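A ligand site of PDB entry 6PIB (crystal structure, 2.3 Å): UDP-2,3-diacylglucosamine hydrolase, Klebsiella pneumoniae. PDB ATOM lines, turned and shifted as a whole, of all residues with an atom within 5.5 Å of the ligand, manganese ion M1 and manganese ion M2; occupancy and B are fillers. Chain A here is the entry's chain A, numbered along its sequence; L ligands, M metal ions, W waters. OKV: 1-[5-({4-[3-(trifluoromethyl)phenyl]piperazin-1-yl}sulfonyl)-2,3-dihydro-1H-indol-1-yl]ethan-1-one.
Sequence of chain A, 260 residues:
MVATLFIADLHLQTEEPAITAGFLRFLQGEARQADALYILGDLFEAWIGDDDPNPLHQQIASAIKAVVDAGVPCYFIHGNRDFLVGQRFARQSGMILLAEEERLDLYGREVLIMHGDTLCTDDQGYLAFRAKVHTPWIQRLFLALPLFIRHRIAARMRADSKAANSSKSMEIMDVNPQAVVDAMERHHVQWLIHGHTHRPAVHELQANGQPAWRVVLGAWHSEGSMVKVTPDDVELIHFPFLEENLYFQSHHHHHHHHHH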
ATOM      1  N   ASP A   9      18.826  21.811  16.587  1.00  0.00           N
ATOM      2  CA  ASP A   9      17.832  21.101  17.388  1.00  0.00           C
ATOM      3  C   ASP A   9      18.294  19.690  17.740  1.00  0.00           C
ATOM      4  O   ASP A   9      17.566  18.709  17.570  1.00  0.00           O
ATOM      5  CB  ASP A   9      16.479  21.080  16.680  1.00  0.00           C
ATOM      6  CG  ASP A   9      15.922  22.473  16.460  1.00  0.00           C
ATOM      7  OD1 ASP A   9      15.664  23.176  17.462  1.00  0.00           O
ATOM      8  OD2 ASP A   9      15.739  22.867  15.286  1.00  0.00           O
ATOM      9  N   HIS A  11      19.307  19.077  20.951  1.00  0.00           N
ATOM     10  CA  HIS A  11      18.799  18.946  22.311  1.00  0.00           C
ATOM     11  C   HIS A  11      19.623  17.955  23.121  1.00  0.00           C
ATOM     12  O   HIS A  11      19.098  17.069  23.803  1.00  0.00           O
ATOM     13  CB  HIS A  11      17.317  18.551  22.299  1.00  0.00           C
ATOM     14  CG  HIS A  11      16.413  19.612  21.755  1.00  0.00           C
ATOM     15  ND1 HIS A  11      15.879  20.612  22.545  1.00  0.00           N
ATOM     16  CD2 HIS A  11      15.957  19.840  20.498  1.00  0.00           C
ATOM     17  CE1 HIS A  11      15.124  21.406  21.802  1.00  0.00           C
ATOM     18  NE2 HIS A  11      15.166  20.958  20.556  1.00  0.00           N
ATOM     19  N   ASP A  42      19.693  25.355  19.666  1.00  0.00           N
ATOM     20  CA  ASP A  42      19.227  24.167  20.371  1.00  0.00           C
ATOM     21  C   ASP A  42      20.217  23.007  20.241  1.00  0.00           C
ATOM     22  O   ASP A  42      19.826  21.851  20.084  1.00  0.00           O
ATOM     23  CB  ASP A  42      17.834  23.748  19.882  1.00  0.00           C
ATOM     24  CG  ASP A  42      16.743  24.665  20.399  1.00  0.00           C
ATOM     25  OD1 ASP A  42      17.083  25.653  21.094  1.00  0.00           O
ATOM     26  OD2 ASP A  42      15.555  24.415  20.101  1.00  0.00           O
ATOM     27  N   GLU A  45      19.809  20.858  25.305  1.00  0.00           N
ATOM     28  CA  GLU A  45      18.444  20.951  25.809  1.00  0.00           C
ATOM     29  C   GLU A  45      18.293  22.095  26.805  1.00  0.00           C
ATOM     30  O   GLU A  45      17.218  22.686  26.918  1.00  0.00           O
ATOM     31  CB  GLU A  45      18.027  19.624  26.434  1.00  0.00           C
ATOM     32  CG  GLU A  45      16.712  19.640  27.197  1.00  0.00           C
ATOM     33  CD  GLU A  45      15.508  19.897  26.306  1.00  0.00           C
ATOM     34  OE1 GLU A  45      15.620  19.693  25.078  1.00  0.00           O
ATOM     35  OE2 GLU A  45      14.450  20.301  26.832  1.00  0.00           O
ATOM     36  N   ALA A  46      19.355  22.420  27.540  1.00  0.00           N
ATOM     37  CA  ALA A  46      19.321  23.464  28.536  1.00  0.00           C
ATOM     38  C   ALA A  46      20.698  24.078  28.683  1.00  0.00           C
ATOM     39  O   ALA A  46      21.711  23.459  28.341  1.00  0.00           O
ATOM     40  CB  ALA A  46      18.818  22.939  29.889  1.00  0.00           C
ATOM     41  N   TRP A  47      20.738  25.301  29.193  1.00  0.00           N
ATOM     42  CA  TRP A  47      22.000  26.001  29.449  1.00  0.00           C
ATOM     43  C   TRP A  47      21.745  27.100  30.469  1.00  0.00           C
ATOM     44  O   TRP A  47      20.880  27.954  30.242  1.00  0.00           O
ATOM     45  CB  TRP A  47      22.584  26.580  28.162  1.00  0.00           C
ATOM     46  CG  TRP A  47      24.049  26.899  28.269  1.00  0.00           C
ATOM     47  CD1 TRP A  47      24.600  28.061  28.723  1.00  0.00           C
ATOM     48  CD2 TRP A  47      25.134  26.041  27.922  1.00  0.00           C
ATOM     49  NE1 TRP A  47      25.968  27.977  28.678  1.00  0.00           N
ATOM     50  CE2 TRP A  47      26.324  26.749  28.189  1.00  0.00           C
ATOM     51  CE3 TRP A  47      25.223  24.738  27.417  1.00  0.00           C
ATOM     52  CZ2 TRP A  47      27.586  26.195  27.969  1.00  0.00           C
ATOM     53  CZ3 TRP A  47      26.478  24.195  27.193  1.00  0.00           C
ATOM     54  CH2 TRP A  47      27.638  24.924  27.472  1.00  0.00           C
ATOM     55  N   ILE A  48      22.486  27.075  31.569  1.00  0.00           N
ATOM     56  CA  ILE A  48      22.347  28.056  32.636  1.00  0.00           C
ATOM     57  C   ILE A  48      23.622  28.861  32.862  1.00  0.00           C
ATOM     58  O   ILE A  48      23.729  29.585  33.842  1.00  0.00           O
ATOM     59  CB  ILE A  48      21.896  27.383  33.954  1.00  0.00           C
ATOM     60  CG1 ILE A  48      22.955  26.399  34.439  1.00  0.00           C
ATOM     61  CG2 ILE A  48      20.553  26.686  33.762  1.00  0.00           C
ATOM     62  CD1 ILE A  48      22.606  25.710  35.740  1.00  0.00           C
ATOM     63  N   GLY A  79      19.743  29.193  20.175  1.00  0.00           N
ATOM     64  CA  GLY A  79      18.372  28.737  20.108  1.00  0.00           C
ATOM     65  C   GLY A  79      17.564  29.218  21.298  1.00  0.00           C
ATOM     66  O   GLY A  79      18.030  29.984  22.134  1.00  0.00           O
ATOM     67  N   ASN A  80      16.323  28.738  21.356  1.00  0.00           N
ATOM     68  CA  ASN A  80      15.461  29.086  22.485  1.00  0.00           C
ATOM     69  C   ASN A  80      15.824  28.330  23.753  1.00  0.00           C
ATOM     70  O   ASN A  80      15.466  28.772  24.844  1.00  0.00           O
ATOM     71  CB  ASN A  80      13.993  28.826  22.130  1.00  0.00           C
ATOM     72  CG  ASN A  80      13.729  27.401  21.709  1.00  0.00           C
ATOM     73  OD1 ASN A  80      14.021  27.014  20.575  1.00  0.00           O
ATOM     74  ND2 ASN A  80      13.176  26.603  22.614  1.00  0.00           N
ATOM     75  N   ARG A  81      16.544  27.221  23.633  1.00  0.00           N
ATOM     76  CA  ARG A  81      16.946  26.429  24.801  1.00  0.00           C
ATOM     77  C   ARG A  81      18.300  26.851  25.348  1.00  0.00           C
ATOM     78  O   ARG A  81      18.490  26.890  26.561  1.00  0.00           O
ATOM     79  CB  ARG A  81      16.969  24.940  24.450  1.00  0.00           C
ATOM     80  CG  ARG A  81      15.682  24.418  23.824  1.00  0.00           C
ATOM     81  CD  ARG A  81      14.525  24.470  24.802  1.00  0.00           C
ATOM     82  NE  ARG A  81      14.855  23.817  26.068  1.00  0.00           N
ATOM     83  CZ  ARG A  81      13.965  23.550  27.021  1.00  0.00           C
ATOM     84  NH1 ARG A  81      12.693  23.883  26.855  1.00  0.00           N
ATOM     85  NH2 ARG A  81      14.347  22.951  28.140  1.00  0.00           N
ATOM     86  N   ASP A  82      19.249  27.168  24.470  1.00  0.00           N
ATOM     87  CA  ASP A  82      20.631  27.433  24.857  1.00  0.00           C
ATOM     88  C   ASP A  82      21.067  28.843  24.471  1.00  0.00           C
ATOM     89  O   ASP A  82      22.158  29.059  23.952  1.00  0.00           O
ATOM     90  CB  ASP A  82      21.574  26.405  24.243  1.00  0.00           C
ATOM     91  CG  ASP A  82      21.360  26.220  22.755  1.00  0.00           C
ATOM     92  OD1 ASP A  82      20.517  26.952  22.179  1.00  0.00           O
ATOM     93  OD2 ASP A  82      22.020  25.353  22.159  1.00  0.00           O
ATOM     94  N   PHE A  83      20.211  29.832  24.739  1.00  0.00           N
ATOM     95  CA  PHE A  83      20.566  31.224  24.456  1.00  0.00           C
ATOM     96  C   PHE A  83      21.601  31.778  25.424  1.00  0.00           C
ATOM     97  O   PHE A  83      22.123  32.873  25.193  1.00  0.00           O
ATOM     98  CB  PHE A  83      19.321  32.108  24.464  1.00  0.00           C
ATOM     99  CG  PHE A  83      18.572  32.078  25.770  1.00  0.00           C
ATOM    100  CD1 PHE A  83      17.584  31.136  26.002  1.00  0.00           C
ATOM    101  CD2 PHE A  83      18.856  33.000  26.761  1.00  0.00           C
ATOM    102  CE1 PHE A  83      16.895  31.116  27.195  1.00  0.00           C
ATOM    103  CE2 PHE A  83      18.176  32.981  27.966  1.00  0.00           C
ATOM    104  CZ  PHE A  83      17.189  32.033  28.179  1.00  0.00           C
ATOM    105  N   LEU A  84      21.917  31.053  26.500  1.00  0.00           N
ATOM    106  CA  LEU A  84      22.912  31.498  27.465  1.00  0.00           C
ATOM    107  C   LEU A  84      24.327  31.021  27.143  1.00  0.00           C
ATOM    108  O   LEU A  84      25.247  31.319  27.903  1.00  0.00           O
ATOM    109  CB  LEU A  84      22.530  31.016  28.880  1.00  0.00           C
ATOM    110  CG  LEU A  84      21.440  31.820  29.599  1.00  0.00           C
ATOM    111  CD1 LEU A  84      21.373  31.422  31.063  1.00  0.00           C
ATOM    112  CD2 LEU A  84      21.689  33.314  29.452  1.00  0.00           C
ATOM    113  N   HIS A 115      17.626  30.634  13.921  1.00  0.00           N
ATOM    114  CA  HIS A 115      17.102  29.480  14.631  1.00  0.00           C
ATOM    115  C   HIS A 115      15.667  29.174  14.208  1.00  0.00           C
ATOM    116  O   HIS A 115      15.305  28.000  14.049  1.00  0.00           O
ATOM    117  CB  HIS A 115      17.172  29.680  16.140  1.00  0.00           C
ATOM    118  CG  HIS A 115      16.647  28.514  16.916  1.00  0.00           C
ATOM    119  ND1 HIS A 115      17.191  27.251  16.834  1.00  0.00           N
ATOM    120  CD2 HIS A 115      15.604  28.415  17.783  1.00  0.00           C
ATOM    121  CE1 HIS A 115      16.518  26.426  17.619  1.00  0.00           C
ATOM    122  NE2 HIS A 115      15.551  27.113  18.207  1.00  0.00           N
ATOM    123  N   ASP A 117      12.809  30.449  15.875  1.00  0.00           N
ATOM    124  CA  ASP A 117      11.821  30.704  16.915  1.00  0.00           C
ATOM    125  C   ASP A 117      11.219  32.102  16.793  1.00  0.00           C
ATOM    126  O   ASP A 117      10.051  32.300  17.139  1.00  0.00           O
ATOM    127  CB  ASP A 117      12.448  30.505  18.296  1.00  0.00           C
ATOM    128  CG  ASP A 117      13.572  31.493  18.567  1.00  0.00           C
ATOM    129  OD1 ASP A 117      14.518  31.553  17.754  1.00  0.00           O
ATOM    130  OD2 ASP A 117      13.514  32.193  19.600  1.00  0.00           O
ATOM    131  N   TYR A 126       5.015  32.359  24.146  1.00  0.00           N
ATOM    132  CA  TYR A 126       6.456  32.201  24.004  1.00  0.00           C
ATOM    133  C   TYR A 126       7.144  33.533  23.762  1.00  0.00           C
ATOM    134  O   TYR A 126       8.248  33.773  24.264  1.00  0.00           O
ATOM    135  CB  TYR A 126       6.799  31.225  22.883  1.00  0.00           C
ATOM    136  CG  TYR A 126       8.253  31.269  22.484  1.00  0.00           C
ATOM    137  CD1 TYR A 126       9.234  30.722  23.302  1.00  0.00           C
ATOM    138  CD2 TYR A 126       8.663  31.883  21.305  1.00  0.00           C
ATOM    139  CE1 TYR A 126      10.579  30.772  22.953  1.00  0.00           C
ATOM    140  CE2 TYR A 126       9.989  31.933  20.943  1.00  0.00           C
ATOM    141  CZ  TYR A 126      10.946  31.374  21.773  1.00  0.00           C
ATOM    142  OH  TYR A 126      12.272  31.424  21.411  1.00  0.00           O
ATOM    143  N   PHE A 129       7.736  35.198  26.996  1.00  0.00           N
ATOM    144  CA  PHE A 129       8.810  34.492  27.693  1.00  0.00           C
ATOM    145  C   PHE A 129      10.161  34.788  27.051  1.00  0.00           C
ATOM    146  O   PHE A 129      11.155  34.991  27.752  1.00  0.00           O
ATOM    147  CB  PHE A 129       8.530  32.985  27.694  1.00  0.00           C
ATOM    148  CG  PHE A 129       9.709  32.144  28.096  1.00  0.00           C
ATOM    149  CD1 PHE A 129       9.961  31.875  29.428  1.00  0.00           C
ATOM    150  CD2 PHE A 129      10.555  31.612  27.135  1.00  0.00           C
ATOM    151  CE1 PHE A 129      11.044  31.096  29.791  1.00  0.00           C
ATOM    152  CE2 PHE A 129      11.637  30.834  27.498  1.00  0.00           C
ATOM    153  CZ  PHE A 129      11.882  30.576  28.826  1.00  0.00           C
ATOM    154  N   VAL A 133      13.496  36.512  29.058  1.00  0.00           N
ATOM    155  CA  VAL A 133      14.775  35.838  29.263  1.00  0.00           C
ATOM    156  C   VAL A 133      15.873  36.335  28.347  1.00  0.00           C
ATOM    157  O   VAL A 133      17.043  35.981  28.551  1.00  0.00           O
ATOM    158  CB  VAL A 133      14.618  34.313  29.104  1.00  0.00           C
ATOM    159  CG1 VAL A 133      13.576  33.778  30.079  1.00  0.00           C
ATOM    160  CG2 VAL A 133      14.245  33.966  27.670  1.00  0.00           C
ATOM    161  N   ILE A 138      18.047  41.000  32.935  1.00  0.00           N
ATOM    162  CA  ILE A 138      17.504  39.762  33.479  1.00  0.00           C
ATOM    163  C   ILE A 138      18.500  38.616  33.324  1.00  0.00           C
ATOM    164  O   ILE A 138      18.585  37.733  34.183  1.00  0.00           O
ATOM    165  CB  ILE A 138      16.145  39.447  32.816  1.00  0.00           C
ATOM    166  CG1 ILE A 138      15.185  40.611  33.021  1.00  0.00           C
ATOM    167  CG2 ILE A 138      15.551  38.160  33.369  1.00  0.00           C
ATOM    168  CD1 ILE A 138      13.811  40.396  32.442  1.00  0.00           C
ATOM    169  N   GLN A 139      19.283  38.628  32.248  1.00  0.00           N
ATOM    170  CA  GLN A 139      20.261  37.565  32.035  1.00  0.00           C
ATOM    171  C   GLN A 139      21.411  37.674  33.021  1.00  0.00           C
ATOM    172  O   GLN A 139      21.788  36.679  33.660  1.00  0.00           O
ATOM    173  CB  GLN A 139      20.798  37.614  30.597  1.00  0.00           C
ATOM    174  CG  GLN A 139      19.822  37.103  29.559  1.00  0.00           C
ATOM    175  CD  GLN A 139      20.462  36.880  28.212  1.00  0.00           C
ATOM    176  OE1 GLN A 139      21.578  37.356  27.964  1.00  0.00           O
ATOM    177  NE2 GLN A 139      19.774  36.162  27.339  1.00  0.00           N
ATOM    178  N   LEU A 141      21.515  39.070  35.856  1.00  0.00           N
ATOM    179  CA  LEU A 141      21.062  38.777  37.207  1.00  0.00           C
ATOM    180  C   LEU A 141      20.963  37.272  37.435  1.00  0.00           C
ATOM    181  O   LEU A 141      21.383  36.773  38.486  1.00  0.00           O
ATOM    182  CB  LEU A 141      19.723  39.454  37.466  1.00  0.00           C
ATOM    183  CG  LEU A 141      19.069  39.117  38.810  1.00  0.00           C
ATOM    184  CD1 LEU A 141      19.543  40.084  39.881  1.00  0.00           C
ATOM    185  CD2 LEU A 141      17.546  39.119  38.707  1.00  0.00           C
ATOM    186  N   PHE A 142      20.401  36.542  36.463  1.00  0.00           N
ATOM    187  CA  PHE A 142      20.350  35.088  36.566  1.00  0.00           C
ATOM    188  C   PHE A 142      21.745  34.489  36.635  1.00  0.00           C
ATOM    189  O   PHE A 142      22.009  33.601  37.461  1.00  0.00           O
ATOM    190  CB  PHE A 142      19.571  34.514  35.378  1.00  0.00           C
ATOM    191  CG  PHE A 142      19.503  33.016  35.346  1.00  0.00           C
ATOM    192  CD1 PHE A 142      18.536  32.329  36.059  1.00  0.00           C
ATOM    193  CD2 PHE A 142      20.389  32.281  34.564  1.00  0.00           C
ATOM    194  CE1 PHE A 142      18.468  30.943  36.014  1.00  0.00           C
ATOM    195  CE2 PHE A 142      20.321  30.896  34.519  1.00  0.00           C
ATOM    196  CZ  PHE A 142      19.357  30.231  35.237  1.00  0.00           C
ATOM    197  N   ILE A 153      16.064  27.101  39.607  1.00  0.00           N
ATOM    198  CA  ILE A 153      15.223  27.992  38.805  1.00  0.00           C
ATOM    199  C   ILE A 153      14.897  27.353  37.463  1.00  0.00           C
ATOM    200  O   ILE A 153      13.733  27.307  37.044  1.00  0.00           O
ATOM    201  CB  ILE A 153      15.917  29.362  38.626  1.00  0.00           C
ATOM    202  CG1 ILE A 153      15.992  30.097  39.966  1.00  0.00           C
ATOM    203  CG2 ILE A 153      15.184  30.197  37.589  1.00  0.00           C
ATOM    204  CD1 ILE A 153      16.645  31.462  39.857  1.00  0.00           C
ATOM    205  N   ALA A 154      15.924  26.857  36.772  1.00  0.00           N
ATOM    206  CA  ALA A 154      15.708  26.273  35.446  1.00  0.00           C
ATOM    207  C   ALA A 154      14.846  25.027  35.519  1.00  0.00           C
ATOM    208  O   ALA A 154      14.027  24.775  34.620  1.00  0.00           O
ATOM    209  CB  ALA A 154      17.058  25.963  34.795  1.00  0.00           C
ATOM    210  N   ALA A 155      14.997  24.228  36.580  1.00  0.00           N
ATOM    211  CA  ALA A 155      14.204  23.013  36.703  1.00  0.00           C
ATOM    212  C   ALA A 155      12.723  23.326  36.878  1.00  0.00           C
ATOM    213  O   ALA A 155      11.871  22.643  36.313  1.00  0.00           O
ATOM    214  CB  ALA A 155      14.720  22.167  37.878  1.00  0.00           C
ATOM    215  N   MET A 157      11.218  26.193  35.924  1.00  0.00           N
ATOM    216  CA  MET A 157      10.727  26.842  34.706  1.00  0.00           C
ATOM    217  C   MET A 157      10.466  25.829  33.597  1.00  0.00           C
ATOM    218  O   MET A 157       9.558  26.032  32.783  1.00  0.00           O
ATOM    219  CB  MET A 157      11.719  27.899  34.240  1.00  0.00           C
ATOM    220  CG  MET A 157      11.841  29.085  35.179  1.00  0.00           C
ATOM    221  SD  MET A 157      13.023  30.318  34.618  1.00  0.00           S
ATOM    222  CE  MET A 157      12.307  30.779  33.044  1.00  0.00           C
ATOM    223  N   ARG A 158      11.238  24.742  33.559  1.00  0.00           N
ATOM    224  CA  ARG A 158      10.946  23.681  32.597  1.00  0.00           C
ATOM    225  C   ARG A 158       9.666  22.943  32.959  1.00  0.00           C
ATOM    226  O   ARG A 158       8.854  22.631  32.078  1.00  0.00           O
ATOM    227  CB  ARG A 158      12.125  22.706  32.515  1.00  0.00           C
ATOM    228  CG  ARG A 158      13.363  23.270  31.834  1.00  0.00           C
ATOM    229  CD  ARG A 158      14.380  22.173  31.530  1.00  0.00           C
ATOM    230  NE  ARG A 158      14.996  21.645  32.746  1.00  0.00           N
ATOM    231  CZ  ARG A 158      16.094  22.147  33.307  1.00  0.00           C
ATOM    232  NH1 ARG A 158      16.697  23.192  32.763  1.00  0.00           N
ATOM    233  NH2 ARG A 158      16.579  21.595  34.411  1.00  0.00           N
ATOM    234  N   SER A 161       6.733  25.364  32.117  1.00  0.00           N
ATOM    235  CA  SER A 161       6.427  25.483  30.698  1.00  0.00           C
ATOM    236  C   SER A 161       5.925  24.174  30.093  1.00  0.00           C
ATOM    237  O   SER A 161       5.185  24.189  29.111  1.00  0.00           O
ATOM    238  CB  SER A 161       7.656  25.985  29.940  1.00  0.00           C
ATOM    239  OG  SER A 161       8.346  24.915  29.323  1.00  0.00           O
ATOM    240  N   HIS A 196      14.136  24.818  14.814  1.00  0.00           N
ATOM    241  CA  HIS A 196      13.179  25.096  15.882  1.00  0.00           C
ATOM    242  C   HIS A 196      11.868  24.330  15.735  1.00  0.00           C
ATOM    243  O   HIS A 196      11.417  23.696  16.695  1.00  0.00           O
ATOM    244  CB  HIS A 196      12.881  26.603  15.969  1.00  0.00           C
ATOM    245  CG  HIS A 196      11.925  26.972  17.061  1.00  0.00           C
ATOM    246  ND1 HIS A 196      12.254  26.908  18.393  1.00  0.00           N
ATOM    247  CD2 HIS A 196      10.642  27.403  17.012  1.00  0.00           C
ATOM    248  CE1 HIS A 196      11.223  27.287  19.118  1.00  0.00           C
ATOM    249  NE2 HIS A 196      10.230  27.594  18.307  1.00  0.00           N
ATOM    250  N   HIS A 198      11.106  21.640  14.068  1.00  0.00           N
ATOM    251  CA  HIS A 198      11.241  20.179  14.024  1.00  0.00           C
ATOM    252  C   HIS A 198      10.437  19.559  12.879  1.00  0.00           C
ATOM    253  O   HIS A 198       9.949  18.433  12.986  1.00  0.00           O
ATOM    254  CB  HIS A 198      10.845  19.538  15.348  1.00  0.00           C
ATOM    255  CG  HIS A 198      11.728  19.911  16.502  1.00  0.00           C
ATOM    256  ND1 HIS A 198      11.687  19.257  17.709  1.00  0.00           N
ATOM    257  CD2 HIS A 198      12.677  20.872  16.616  1.00  0.00           C
ATOM    258  CE1 HIS A 198      12.568  19.802  18.528  1.00  0.00           C
ATOM    259  NE2 HIS A 198      13.185  20.786  17.889  1.00  0.00           N
ATOM    260  N   ALA A 219      14.850  17.879  13.871  1.00  0.00           N
ATOM    261  CA  ALA A 219      15.436  17.615  15.173  1.00  0.00           C
ATOM    262  C   ALA A 219      16.053  16.219  15.201  1.00  0.00           C
ATOM    263  O   ALA A 219      15.639  15.313  14.474  1.00  0.00           O
ATOM    264  CB  ALA A 219      14.375  17.731  16.267  1.00  0.00           C
HETATM  265  C13 OKV L   1      15.345  27.174  28.253  1.00  0.00           C
HETATM  266  C15 OKV L   1      12.958  27.205  27.927  1.00  0.00           C
HETATM  267  C17 OKV L   1      13.869  26.445  30.028  1.00  0.00           C
HETATM  268  C21 OKV L   1      11.363  27.843  25.928  1.00  0.00           C
HETATM  269  C24 OKV L   1      16.081  32.336  33.406  1.00  0.00           C
HETATM  270  C26 OKV L   1      16.893  34.563  33.088  1.00  0.00           C
HETATM  271  C28 OKV L   1      15.207  34.148  34.916  1.00  0.00           C
HETATM  272  C01 OKV L   1      17.685  32.788  31.685  1.00  0.00           C
HETATM  273  C02 OKV L   1      16.884  31.896  32.361  1.00  0.00           C
HETATM  274  C04 OKV L   1      16.260  29.560  32.930  1.00  0.00           C
HETATM  275  C05 OKV L   1      15.904  28.270  32.198  1.00  0.00           C
HETATM  276  C07 OKV L   1      17.637  28.703  30.548  1.00  0.00           C
HETATM  277  C08 OKV L   1      18.027  29.992  31.262  1.00  0.00           C
HETATM  278  C12 OKV L   1      15.163  26.682  29.555  1.00  0.00           C
HETATM  279  C14 OKV L   1      14.252  27.440  27.444  1.00  0.00           C
HETATM  280  C16 OKV L   1      12.758  26.711  29.207  1.00  0.00           C
HETATM  281  C18 OKV L   1      11.271  26.544  29.482  1.00  0.00           C
HETATM  282  C19 OKV L   1      10.581  27.041  28.247  1.00  0.00           C
HETATM  283  C23 OKV L   1       9.915  27.962  25.462  1.00  0.00           C
HETATM  284  C25 OKV L   1      16.090  33.662  33.767  1.00  0.00           C
HETATM  285  C27 OKV L   1      17.688  34.135  32.039  1.00  0.00           C
HETATM  286  F29 OKV L   1      13.943  34.240  34.498  1.00  0.00           F
HETATM  287  F30 OKV L   1      15.625  35.340  35.338  1.00  0.00           F
HETATM  288  F31 OKV L   1      15.272  33.279  35.926  1.00  0.00           F
HETATM  289  N03 OKV L   1      16.868  30.542  32.008  1.00  0.00           N
HETATM  290  N06 OKV L   1      17.043  27.738  31.466  1.00  0.00           N
HETATM  291  N20 OKV L   1      11.620  27.389  27.285  1.00  0.00           N
HETATM  292  O10 OKV L   1      17.715  25.945  29.752  1.00  0.00           O
HETATM  293  O11 OKV L   1      16.277  25.264  31.538  1.00  0.00           O
HETATM  294  O22 OKV L   1      12.258  28.109  25.206  1.00  0.00           O
HETATM  295  S09 OKV L   1      16.597  26.345  30.598  1.00  0.00           S
HETATM  296 MN    MN M   1      14.089  25.709  19.199  1.00  0.00          MN
HETATM  297 MN    MN M   2      14.601  22.283  18.772  1.00  0.00          MN
HETATM  298  O   HOH W   1      13.166  23.791  19.246  1.00  0.00           O
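The nearest printed residue that does not touch manganese ion M2 is His 196 (4.1 Å).
O10 of the ligand sits at hydrogen-bond distance from N of Trp 47. An oxygen (O11) of the ligand sits at hydrogen-bond distance from the guanidinium group (NH1) of Arg 158, 2.4 Å away. The side-chain amide nitrogen of Asn 80 is in hydrogen-bond range of an oxygen (O22) of the ligand, 3.1 Å away.
Five residues have an atom within 4 Å of manganese ion M1: Asp 9, Asp 42, Asn 80, His 115 and His 196. Along chain A the residues within 4 Å of manganese ion M1 span positions 9 to 196. The nearest printed residue that does not touch manganese ion M1 is His 11 (5.1 Å).
An oxygen (O10) of the ligand lies close to the backbone carbonyl oxygen (O) of Arg 81 (3.4 Å). CA of Ala 46 touches O10 of the ligand, 3.2 Å away. Phe 83 touches the ligand. CD1 of Leu 84 touches C08 of the ligand, at 3.6 Å. Tyr 126 touches the ligand. Phe 129 touches the ligand. Val 133 touches the ligand. Ile 138 touches the ligand. CD1 of Phe 142 touches F31 of the ligand, 3.4 Å away. Ile 153 touches the ligand (CG2 to F31, 3.5 Å). CB of Ala 154 touches O11 of the ligand, 3.4 Å away. Met 157 touches the ligand (SD to C04, 3.7 Å). Ser 161 touches the ligand (OG to C19, 3.3 Å). Of the 31 residues printed, 16 come within 4 Å of the ligand. The nearest printed residue that does not touch the ligand is Gln 139 (4.3 Å).
Manganese ion M2 is bound by OD1 of Asp 9, water W1, NE2 of His 198, NE2 of His 11 and OD2 of Asp 42.
The guanidinium group (NH2) of Arg 81 is in salt-bridge range of the side-chain carboxylate (OE2) of Glu 45 (3.0 Å). The side-chain carboxylate of Asp 42 lies within hydrogen-bond range of the backbone NH of Arg 81, at 3.0 Å. The backbone carbonyl oxygen of Val 133 lies within hydrogen-bond range of the side-chain amide nitrogen of Gln 139 (3.0 Å). ND1 of His 11 lies within hydrogen-bond range of OE1 of Glu 45. N of Asp 42 lies within hydrogen-bond range of OD1 of Asp 82, at 3.1 Å. N of His 196 sits at hydrogen-bond distance from OD2 of Asp 9 (2.6 Å).
Manganese ion M1 is bound by OD1 of Asn 80 (1.9 Å), water W1 (2.1 Å), OD2 of Asp 42 (2.2 Å), NE2 of His 115 (2.3 Å) and ND1 of His 196 (2.3 Å). Manganese ion M1 has five donor atoms within binding distance.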
